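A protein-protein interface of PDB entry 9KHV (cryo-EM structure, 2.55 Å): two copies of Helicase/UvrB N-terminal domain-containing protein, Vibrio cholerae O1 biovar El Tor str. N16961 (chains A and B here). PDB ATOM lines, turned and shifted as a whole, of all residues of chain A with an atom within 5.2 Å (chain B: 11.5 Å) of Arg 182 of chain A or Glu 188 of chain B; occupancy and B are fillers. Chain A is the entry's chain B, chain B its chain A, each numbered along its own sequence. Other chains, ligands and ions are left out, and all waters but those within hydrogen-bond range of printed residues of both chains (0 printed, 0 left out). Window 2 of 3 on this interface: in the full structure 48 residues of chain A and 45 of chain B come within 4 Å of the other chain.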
ATOM      1  N   ASP A 152     -10.722   9.445  23.239  1.00  0.00           N
ATOM      2  CA  ASP A 152      -9.528   9.749  22.455  1.00  0.00           C
ATOM      3  C   ASP A 152      -8.399   8.770  22.743  1.00  0.00           C
ATOM      4  O   ASP A 152      -7.574   8.503  21.863  1.00  0.00           O
ATOM      5  CB  ASP A 152      -9.069  11.180  22.724  1.00  0.00           C
ATOM      6  CG  ASP A 152     -10.048  12.213  22.210  1.00  0.00           C
ATOM      7  OD1 ASP A 152     -11.223  12.178  22.630  1.00  0.00           O
ATOM      8  OD2 ASP A 152      -9.645  13.060  21.387  1.00  0.00           O
ATOM      9  N   SER A 175      -7.693  14.968  13.975  1.00  0.00           N
ATOM     10  CA  SER A 175      -7.469  16.174  14.761  1.00  0.00           C
ATOM     11  C   SER A 175      -8.657  17.120  14.661  1.00  0.00           C
ATOM     12  O   SER A 175      -9.076  17.710  15.665  1.00  0.00           O
ATOM     13  CB  SER A 175      -6.188  16.867  14.300  1.00  0.00           C
ATOM     14  OG  SER A 175      -6.401  17.567  13.087  1.00  0.00           O
ATOM     15  N   ALA A 176      -9.219  17.272  13.458  1.00  0.00           N
ATOM     16  CA  ALA A 176     -10.396  18.118  13.296  1.00  0.00           C
ATOM     17  C   ALA A 176     -11.565  17.603  14.124  1.00  0.00           C
ATOM     18  O   ALA A 176     -12.259  18.381  14.791  1.00  0.00           O
ATOM     19  CB  ALA A 176     -10.781  18.203  11.820  1.00  0.00           C
ATOM     20  N   SER A 178     -11.452  15.609  16.806  1.00  0.00           N
ATOM     21  CA  SER A 178     -11.148  15.762  18.226  1.00  0.00           C
ATOM     22  C   SER A 178     -11.333  17.206  18.675  1.00  0.00           C
ATOM     23  O   SER A 178     -11.808  17.462  19.787  1.00  0.00           O
ATOM     24  CB  SER A 178      -9.727  15.287  18.514  1.00  0.00           C
ATOM     25  OG  SER A 178      -8.803  15.910  17.643  1.00  0.00           O
ATOM     26  N   GLY A 179     -10.957  18.164  17.827  1.00  0.00           N
ATOM     27  CA  GLY A 179     -11.210  19.558  18.148  1.00  0.00           C
ATOM     28  C   GLY A 179     -12.691  19.879  18.211  1.00  0.00           C
ATOM     29  O   GLY A 179     -13.138  20.630  19.080  1.00  0.00           O
ATOM     30  N   LEU A 180     -13.472  19.317  17.286  1.00  0.00           N
ATOM     31  CA  LEU A 180     -14.916  19.520  17.312  1.00  0.00           C
ATOM     32  C   LEU A 180     -15.553  18.917  18.557  1.00  0.00           C
ATOM     33  O   LEU A 180     -16.526  19.468  19.081  1.00  0.00           O
ATOM     34  CB  LEU A 180     -15.553  18.919  16.061  1.00  0.00           C
ATOM     35  CG  LEU A 180     -15.886  19.867  14.914  1.00  0.00           C
ATOM     36  CD1 LEU A 180     -16.543  19.098  13.783  1.00  0.00           C
ATOM     37  CD2 LEU A 180     -16.783  20.989  15.393  1.00  0.00           C
ATOM     38  N   ARG A 181     -15.028  17.785  19.033  1.00  0.00           N
ATOM     39  CA  ARG A 181     -15.640  17.096  20.167  1.00  0.00           C
ATOM     40  C   ARG A 181     -15.616  17.951  21.427  1.00  0.00           C
ATOM     41  O   ARG A 181     -16.608  18.012  22.164  1.00  0.00           O
ATOM     42  CB  ARG A 181     -14.932  15.764  20.415  1.00  0.00           C
ATOM     43  CG  ARG A 181     -15.274  14.676  19.419  1.00  0.00           C
ATOM     44  CD  ARG A 181     -14.472  13.414  19.687  1.00  0.00           C
ATOM     45  NE  ARG A 181     -15.153  12.517  20.612  1.00  0.00           N
ATOM     46  CZ  ARG A 181     -14.647  11.374  21.056  1.00  0.00           C
ATOM     47  NH1 ARG A 181     -13.449  10.958  20.682  1.00  0.00           N
ATOM     48  NH2 ARG A 181     -15.364  10.630  21.892  1.00  0.00           N
ATOM     49  N   ARG A 182     -14.491  18.616  21.698  1.00  0.00           N
ATOM     50  CA  ARG A 182     -14.379  19.403  22.923  1.00  0.00           C
ATOM     51  C   ARG A 182     -15.263  20.642  22.889  1.00  0.00           C
ATOM     52  O   ARG A 182     -15.667  21.141  23.945  1.00  0.00           O
ATOM     53  CB  ARG A 182     -12.924  19.807  23.158  1.00  0.00           C
ATOM     54  CG  ARG A 182     -12.107  18.771  23.903  1.00  0.00           C
ATOM     55  CD  ARG A 182     -11.125  18.090  22.973  1.00  0.00           C
ATOM     56  NE  ARG A 182     -10.211  19.046  22.360  1.00  0.00           N
ATOM     57  CZ  ARG A 182      -9.006  18.738  21.901  1.00  0.00           C
ATOM     58  NH1 ARG A 182      -8.532  17.506  21.975  1.00  0.00           N
ATOM     59  NH2 ARG A 182      -8.258  19.692  21.354  1.00  0.00           N
ATOM     60  N   HIS A 183     -15.572  21.150  21.699  1.00  0.00           N
ATOM     61  CA  HIS A 183     -16.358  22.370  21.535  1.00  0.00           C
ATOM     62  C   HIS A 183     -17.812  22.066  21.204  1.00  0.00           C
ATOM     63  O   HIS A 183     -18.440  22.781  20.418  1.00  0.00           O
ATOM     64  CB  HIS A 183     -15.742  23.269  20.465  1.00  0.00           C
ATOM     65  CG  HIS A 183     -14.307  23.623  20.714  1.00  0.00           C
ATOM     66  ND1 HIS A 183     -13.339  22.683  20.997  1.00  0.00           N
ATOM     67  CD2 HIS A 183     -13.678  24.822  20.721  1.00  0.00           C
ATOM     68  CE1 HIS A 183     -12.177  23.287  21.168  1.00  0.00           C
ATOM     69  NE2 HIS A 183     -12.355  24.585  21.006  1.00  0.00           N
ATOM     70  N   ALA A 184     -18.373  21.008  21.788  1.00  0.00           N
ATOM     71  CA  ALA A 184     -19.739  20.614  21.469  1.00  0.00           C
ATOM     72  C   ALA A 184     -20.733  21.631  22.012  1.00  0.00           C
ATOM     73  O   ALA A 184     -21.195  21.525  23.153  1.00  0.00           O
ATOM     74  CB  ALA A 184     -20.042  19.221  22.023  1.00  0.00           C
ATOM     75  N   LEU B 148     -16.369  30.509   2.079  1.00  0.00           N
ATOM     76  CA  LEU B 148     -16.373  31.178   3.377  1.00  0.00           C
ATOM     77  C   LEU B 148     -16.352  32.697   3.291  1.00  0.00           C
ATOM     78  O   LEU B 148     -16.568  33.352   4.316  1.00  0.00           O
ATOM     79  CB  LEU B 148     -15.195  30.695   4.221  1.00  0.00           C
ATOM     80  CG  LEU B 148     -15.570  29.698   5.316  1.00  0.00           C
ATOM     81  CD1 LEU B 148     -16.456  28.613   4.775  1.00  0.00           C
ATOM     82  CD2 LEU B 148     -14.316  29.094   5.915  1.00  0.00           C
ATOM     83  N   LEU B 180     -21.573  26.192  11.878  1.00  0.00           N
ATOM     84  CA  LEU B 180     -20.140  26.244  12.147  1.00  0.00           C
ATOM     85  C   LEU B 180     -19.601  27.660  11.983  1.00  0.00           C
ATOM     86  O   LEU B 180     -18.741  28.101  12.754  1.00  0.00           O
ATOM     87  CB  LEU B 180     -19.401  25.283  11.219  1.00  0.00           C
ATOM     88  CG  LEU B 180     -19.038  23.910  11.777  1.00  0.00           C
ATOM     89  CD1 LEU B 180     -18.287  23.105  10.734  1.00  0.00           C
ATOM     90  CD2 LEU B 180     -18.225  24.042  13.049  1.00  0.00           C
ATOM     91  N   ARG B 181     -20.091  28.382  10.973  1.00  0.00           N
ATOM     92  CA  ARG B 181     -19.621  29.738  10.707  1.00  0.00           C
ATOM     93  C   ARG B 181     -19.941  30.669  11.866  1.00  0.00           C
ATOM     94  O   ARG B 181     -19.095  31.466  12.290  1.00  0.00           O
ATOM     95  CB  ARG B 181     -20.251  30.267   9.420  1.00  0.00           C
ATOM     96  CG  ARG B 181     -19.615  29.765   8.144  1.00  0.00           C
ATOM     97  CD  ARG B 181     -20.350  30.314   6.934  1.00  0.00           C
ATOM     98  NE  ARG B 181     -19.779  31.573   6.473  1.00  0.00           N
ATOM     99  CZ  ARG B 181     -20.271  32.300   5.480  1.00  0.00           C
ATOM    100  NH1 ARG B 181     -21.355  31.927   4.822  1.00  0.00           N
ATOM    101  NH2 ARG B 181     -19.658  33.429   5.137  1.00  0.00           N
ATOM    102  N   HIS B 183     -20.162  30.006  14.854  1.00  0.00           N
ATOM    103  CA  HIS B 183     -19.444  29.570  16.048  1.00  0.00           C
ATOM    104  C   HIS B 183     -17.951  29.416  15.773  1.00  0.00           C
ATOM    105  O   HIS B 183     -17.338  28.413  16.138  1.00  0.00           O
ATOM    106  CB  HIS B 183     -20.022  28.261  16.579  1.00  0.00           C
ATOM    107  CG  HIS B 183     -21.392  28.398  17.164  1.00  0.00           C
ATOM    108  ND1 HIS B 183     -21.654  29.183  18.265  1.00  0.00           N
ATOM    109  CD2 HIS B 183     -22.576  27.850  16.802  1.00  0.00           C
ATOM    110  CE1 HIS B 183     -22.941  29.114  18.556  1.00  0.00           C
ATOM    111  NE2 HIS B 183     -23.524  28.312  17.683  1.00  0.00           N
ATOM    112  N   ALA B 184     -17.349  30.413  15.125  1.00  0.00           N
ATOM    113  CA  ALA B 184     -15.944  30.328  14.750  1.00  0.00           C
ATOM    114  C   ALA B 184     -15.041  30.493  15.966  1.00  0.00           C
ATOM    115  O   ALA B 184     -14.615  31.606  16.293  1.00  0.00           O
ATOM    116  CB  ALA B 184     -15.606  31.378  13.690  1.00  0.00           C
ATOM    117  N   SER B 185     -14.747  29.384  16.635  1.00  0.00           N
ATOM    118  CA  SER B 185     -13.867  29.353  17.795  1.00  0.00           C
ATOM    119  C   SER B 185     -12.429  29.142  17.320  1.00  0.00           C
ATOM    120  O   SER B 185     -12.112  29.358  16.148  1.00  0.00           O
ATOM    121  CB  SER B 185     -14.333  28.272  18.775  1.00  0.00           C
ATOM    122  OG  SER B 185     -15.639  28.543  19.252  1.00  0.00           O
ATOM    123  N   ASN B 186     -11.539  28.750  18.234  1.00  0.00           N
ATOM    124  CA  ASN B 186     -10.140  28.442  17.953  1.00  0.00           C
ATOM    125  C   ASN B 186     -10.019  27.521  16.742  1.00  0.00           C
ATOM    126  O   ASN B 186     -10.962  26.783  16.432  1.00  0.00           O
ATOM    127  CB  ASN B 186      -9.486  27.805  19.183  1.00  0.00           C
ATOM    128  CG  ASN B 186      -8.516  28.742  19.878  1.00  0.00           C
ATOM    129  OD1 ASN B 186      -8.379  29.905  19.499  1.00  0.00           O
ATOM    130  ND2 ASN B 186      -7.835  28.237  20.900  1.00  0.00           N
ATOM    131  N   PRO B 187      -8.867  27.529  16.034  1.00  0.00           N
ATOM    132  CA  PRO B 187      -8.764  26.825  14.742  1.00  0.00           C
ATOM    133  C   PRO B 187      -9.218  25.372  14.746  1.00  0.00           C
ATOM    134  O   PRO B 187      -9.409  24.781  13.675  1.00  0.00           O
ATOM    135  CB  PRO B 187      -7.267  26.922  14.406  1.00  0.00           C
ATOM    136  CG  PRO B 187      -6.600  27.525  15.611  1.00  0.00           C
ATOM    137  CD  PRO B 187      -7.645  28.285  16.344  1.00  0.00           C
ATOM    138  N   GLU B 188      -9.394  24.786  15.934  1.00  0.00           N
ATOM    139  CA  GLU B 188      -9.932  23.433  16.024  1.00  0.00           C
ATOM    140  C   GLU B 188     -11.278  23.325  15.320  1.00  0.00           C
ATOM    141  O   GLU B 188     -11.603  22.274  14.754  1.00  0.00           O
ATOM    142  CB  GLU B 188     -10.061  23.018  17.490  1.00  0.00           C
ATOM    143  CG  GLU B 188      -8.738  22.676  18.172  1.00  0.00           C
ATOM    144  CD  GLU B 188      -8.239  21.275  17.856  1.00  0.00           C
ATOM    145  OE1 GLU B 188      -8.413  20.809  16.711  1.00  0.00           O
ATOM    146  OE2 GLU B 188      -7.668  20.636  18.763  1.00  0.00           O
ATOM    147  N   VAL B 189     -12.069  24.393  15.349  1.00  0.00           N
ATOM    148  CA  VAL B 189     -13.280  24.469  14.542  1.00  0.00           C
ATOM    149  C   VAL B 189     -12.964  24.853  13.095  1.00  0.00           C
ATOM    150  O   VAL B 189     -13.653  24.404  12.171  1.00  0.00           O
ATOM    151  CB  VAL B 189     -14.260  25.467  15.189  1.00  0.00           C
ATOM    152  CG1 VAL B 189     -15.331  25.912  14.205  1.00  0.00           C
ATOM    153  CG2 VAL B 189     -14.886  24.862  16.434  1.00  0.00           C
ATOM    154  N   LYS B 190     -11.911  25.646  12.882  1.00  0.00           N
ATOM    155  CA  LYS B 190     -11.659  26.228  11.569  1.00  0.00           C
ATOM    156  C   LYS B 190     -11.223  25.179  10.552  1.00  0.00           C
ATOM    157  O   LYS B 190     -11.569  25.280   9.369  1.00  0.00           O
ATOM    158  CB  LYS B 190     -10.607  27.331  11.683  1.00  0.00           C
ATOM    159  CG  LYS B 190     -11.173  28.743  11.638  1.00  0.00           C
ATOM    160  CD  LYS B 190     -11.927  29.014  10.346  1.00  0.00           C
ATOM    161  CE  LYS B 190     -11.054  28.758   9.130  1.00  0.00           C
ATOM    162  NZ  LYS B 190     -11.658  29.298   7.885  1.00  0.00           N
ATOM    163  N   ILE B 191     -10.454  24.175  10.979  1.00  0.00           N
ATOM    164  CA  ILE B 191     -10.036  23.127  10.045  1.00  0.00           C
ATOM    165  C   ILE B 191     -11.252  22.381   9.505  1.00  0.00           C
ATOM    166  O   ILE B 191     -11.396  22.172   8.289  1.00  0.00           O
ATOM    167  CB  ILE B 191      -9.040  22.163  10.716  1.00  0.00           C
ATOM    168  CG1 ILE B 191      -8.091  22.922  11.643  1.00  0.00           C
ATOM    169  CG2 ILE B 191      -8.261  21.384   9.668  1.00  0.00           C
ATOM    170  CD1 ILE B 191      -7.074  23.774  10.914  1.00  0.00           C
ATOM    171  N   SER B 192     -12.150  21.976  10.405  1.00  0.00           N
ATOM    172  CA  SER B 192     -13.366  21.296   9.979  1.00  0.00           C
ATOM    173  C   SER B 192     -14.220  22.206   9.109  1.00  0.00           C
ATOM    174  O   SER B 192     -14.801  21.759   8.113  1.00  0.00           O
ATOM    175  CB  SER B 192     -14.154  20.818  11.198  1.00  0.00           C
ATOM    176  OG  SER B 192     -13.966  21.688  12.298  1.00  0.00           O
ATOM    177  N   LEU B 193     -14.306  23.490   9.468  1.00  0.00           N
ATOM    178  CA  LEU B 193     -15.086  24.422   8.665  1.00  0.00           C
ATOM    179  C   LEU B 193     -14.544  24.510   7.245  1.00  0.00           C
ATOM    180  O   LEU B 193     -15.314  24.503   6.280  1.00  0.00           O
ATOM    181  CB  LEU B 193     -15.099  25.800   9.323  1.00  0.00           C
ATOM    182  CG  LEU B 193     -15.921  26.877   8.618  1.00  0.00           C
ATOM    183  CD1 LEU B 193     -17.349  26.416   8.402  1.00  0.00           C
ATOM    184  CD2 LEU B 193     -15.889  28.169   9.410  1.00  0.00           C
ATOM    185  N   ASN B 194     -13.219  24.575   7.098  1.00  0.00           N
ATOM    186  CA  ASN B 194     -12.620  24.632   5.768  1.00  0.00           C
ATOM    187  C   ASN B 194     -12.901  23.364   4.971  1.00  0.00           C
ATOM    188  O   ASN B 194     -13.235  23.429   3.778  1.00  0.00           O
ATOM    189  CB  ASN B 194     -11.115  24.864   5.885  1.00  0.00           C
ATOM    190  CG  ASN B 194     -10.746  26.327   5.805  1.00  0.00           C
ATOM    191  OD1 ASN B 194     -10.127  26.872   6.718  1.00  0.00           O
ATOM    192  ND2 ASN B 194     -11.124  26.975   4.711  1.00  0.00           N
ATOM    193  N   ARG B 195     -12.767  22.197   5.609  1.00  0.00           N
ATOM    194  CA  ARG B 195     -13.015  20.944   4.898  1.00  0.00           C
ATOM    195  C   ARG B 195     -14.457  20.866   4.405  1.00  0.00           C
ATOM    196  O   ARG B 195     -14.717  20.545   3.231  1.00  0.00           O
ATOM    197  CB  ARG B 195     -12.688  19.756   5.802  1.00  0.00           C
ATOM    198  CG  ARG B 195     -11.226  19.656   6.198  1.00  0.00           C
ATOM    199  CD  ARG B 195     -10.980  18.461   7.107  1.00  0.00           C
ATOM    200  NE  ARG B 195     -10.462  17.313   6.374  1.00  0.00           N
ATOM    201  CZ  ARG B 195     -11.216  16.355   5.850  1.00  0.00           C
ATOM    202  NH1 ARG B 195     -12.533  16.375   5.963  1.00  0.00           N
ATOM    203  NH2 ARG B 195     -10.633  15.355   5.197  1.00  0.00           N
ATOM    204  N   GLN B 196     -15.413  21.171   5.285  1.00  0.00           N
ATOM    205  CA  GLN B 196     -16.811  21.121   4.875  1.00  0.00           C
ATOM    206  C   GLN B 196     -17.131  22.187   3.843  1.00  0.00           C
ATOM    207  O   GLN B 196     -17.973  21.960   2.969  1.00  0.00           O
ATOM    208  CB  GLN B 196     -17.742  21.249   6.081  1.00  0.00           C
ATOM    209  CG  GLN B 196     -17.315  20.438   7.280  1.00  0.00           C
ATOM    210  CD  GLN B 196     -16.818  19.061   6.898  1.00  0.00           C
ATOM    211  OE1 GLN B 196     -17.490  18.321   6.178  1.00  0.00           O
ATOM    212  NE2 GLN B 196     -15.628  18.710   7.371  1.00  0.00           N
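The backbone carbonyl oxygen of Glu 188 of chain B lies within hydrogen-bond range of the side-chain hydroxyl of Ser 192 of chain B. The side-chain hydroxyl of Ser 192 of chain B is in hydrogen-bond range of the backbone carbonyl oxygen of Val 189 of chain B (2.7 Å). NE2 of Gln 196 of chain B lies close to O of Ser 192 of chain B (3.2 Å). The backbone carbonyl oxygen (O) of Ser 175 of chain A is in hydrogen-bond range of the side-chain hydroxyl (OG) of Ser 178 of chain A. The backbone carbonyl oxygen (O) of Ser 178 of chain A sits close to the guanidinium group (NE) of Arg 182 of chain A. A ring nitrogen (ND1) of His 183 of chain A lies within hydrogen-bond range of the backbone carbonyl oxygen (O) of Gly 179 of chain A (2.8 Å).
Ala 176 of chain A touches Glu 188 of chain B (O to O, 3.9 Å). OE1 of Glu 188 of chain B touches CA of Gly 179 of chain A, at 3.4 Å. CG of Leu 180 of chain A touches OG of Ser 192 of chain B, at 3.7 Å.
The guanidinium group of Arg 182 of chain A lies within salt-bridge range of the side-chain carboxylate of Glu 188 of chain B, at 2.8 Å. OE1 of Glu 188 of chain B sits close to O of Ser 175 of chain A.
Of chain B, only Glu 188 comes within 4 Å of Ser 175 of chain A. Ala 176 of chain A touches one residue of chain B. No residue of chain B comes within 4 Å of Ser 178 of chain A. Printed residues of chain B within 4 Å of Gly 179 of chain A: Glu 188. Of chain B, only Ser 192 comes within 4 Å of Leu 180 of chain A. Of chain B, only Glu 188 (2.8 Å) comes within 4 Å of Arg 182 of chain A. Ile 191 of chain B touches none of the printed residues of chain A. Printed residues of chain A within 4 Å of Ser 192 of chain B: Leu 180. The nearest residue of chain B that does not touch Arg 182 of chain A is Val 189 of chain B (7.7 Å). The nearest residue of chain A that does not touch Glu 188 of chain B is His 183 of chain A (4.3 Å).
4 positions are printed for both chains. Of the 5 pairs that touch across the chains among the printed residues, none has its exchanged pair printed and touching as well.
Of the 10 printed residues of chain A, 5 touch a printed residue of chain B. Printed residues of chain A that touch a printed residue of chain B: Ser 175, Ala 176, Gly 179, Leu 180 and Arg 182. Among the printed residues, Asp or Glu carboxylates within 4 Å of a Lys or Arg side-chain nitrogen of the other chain: Arg 182 of chain A with Glu 188 of chain B (2.8 Å).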
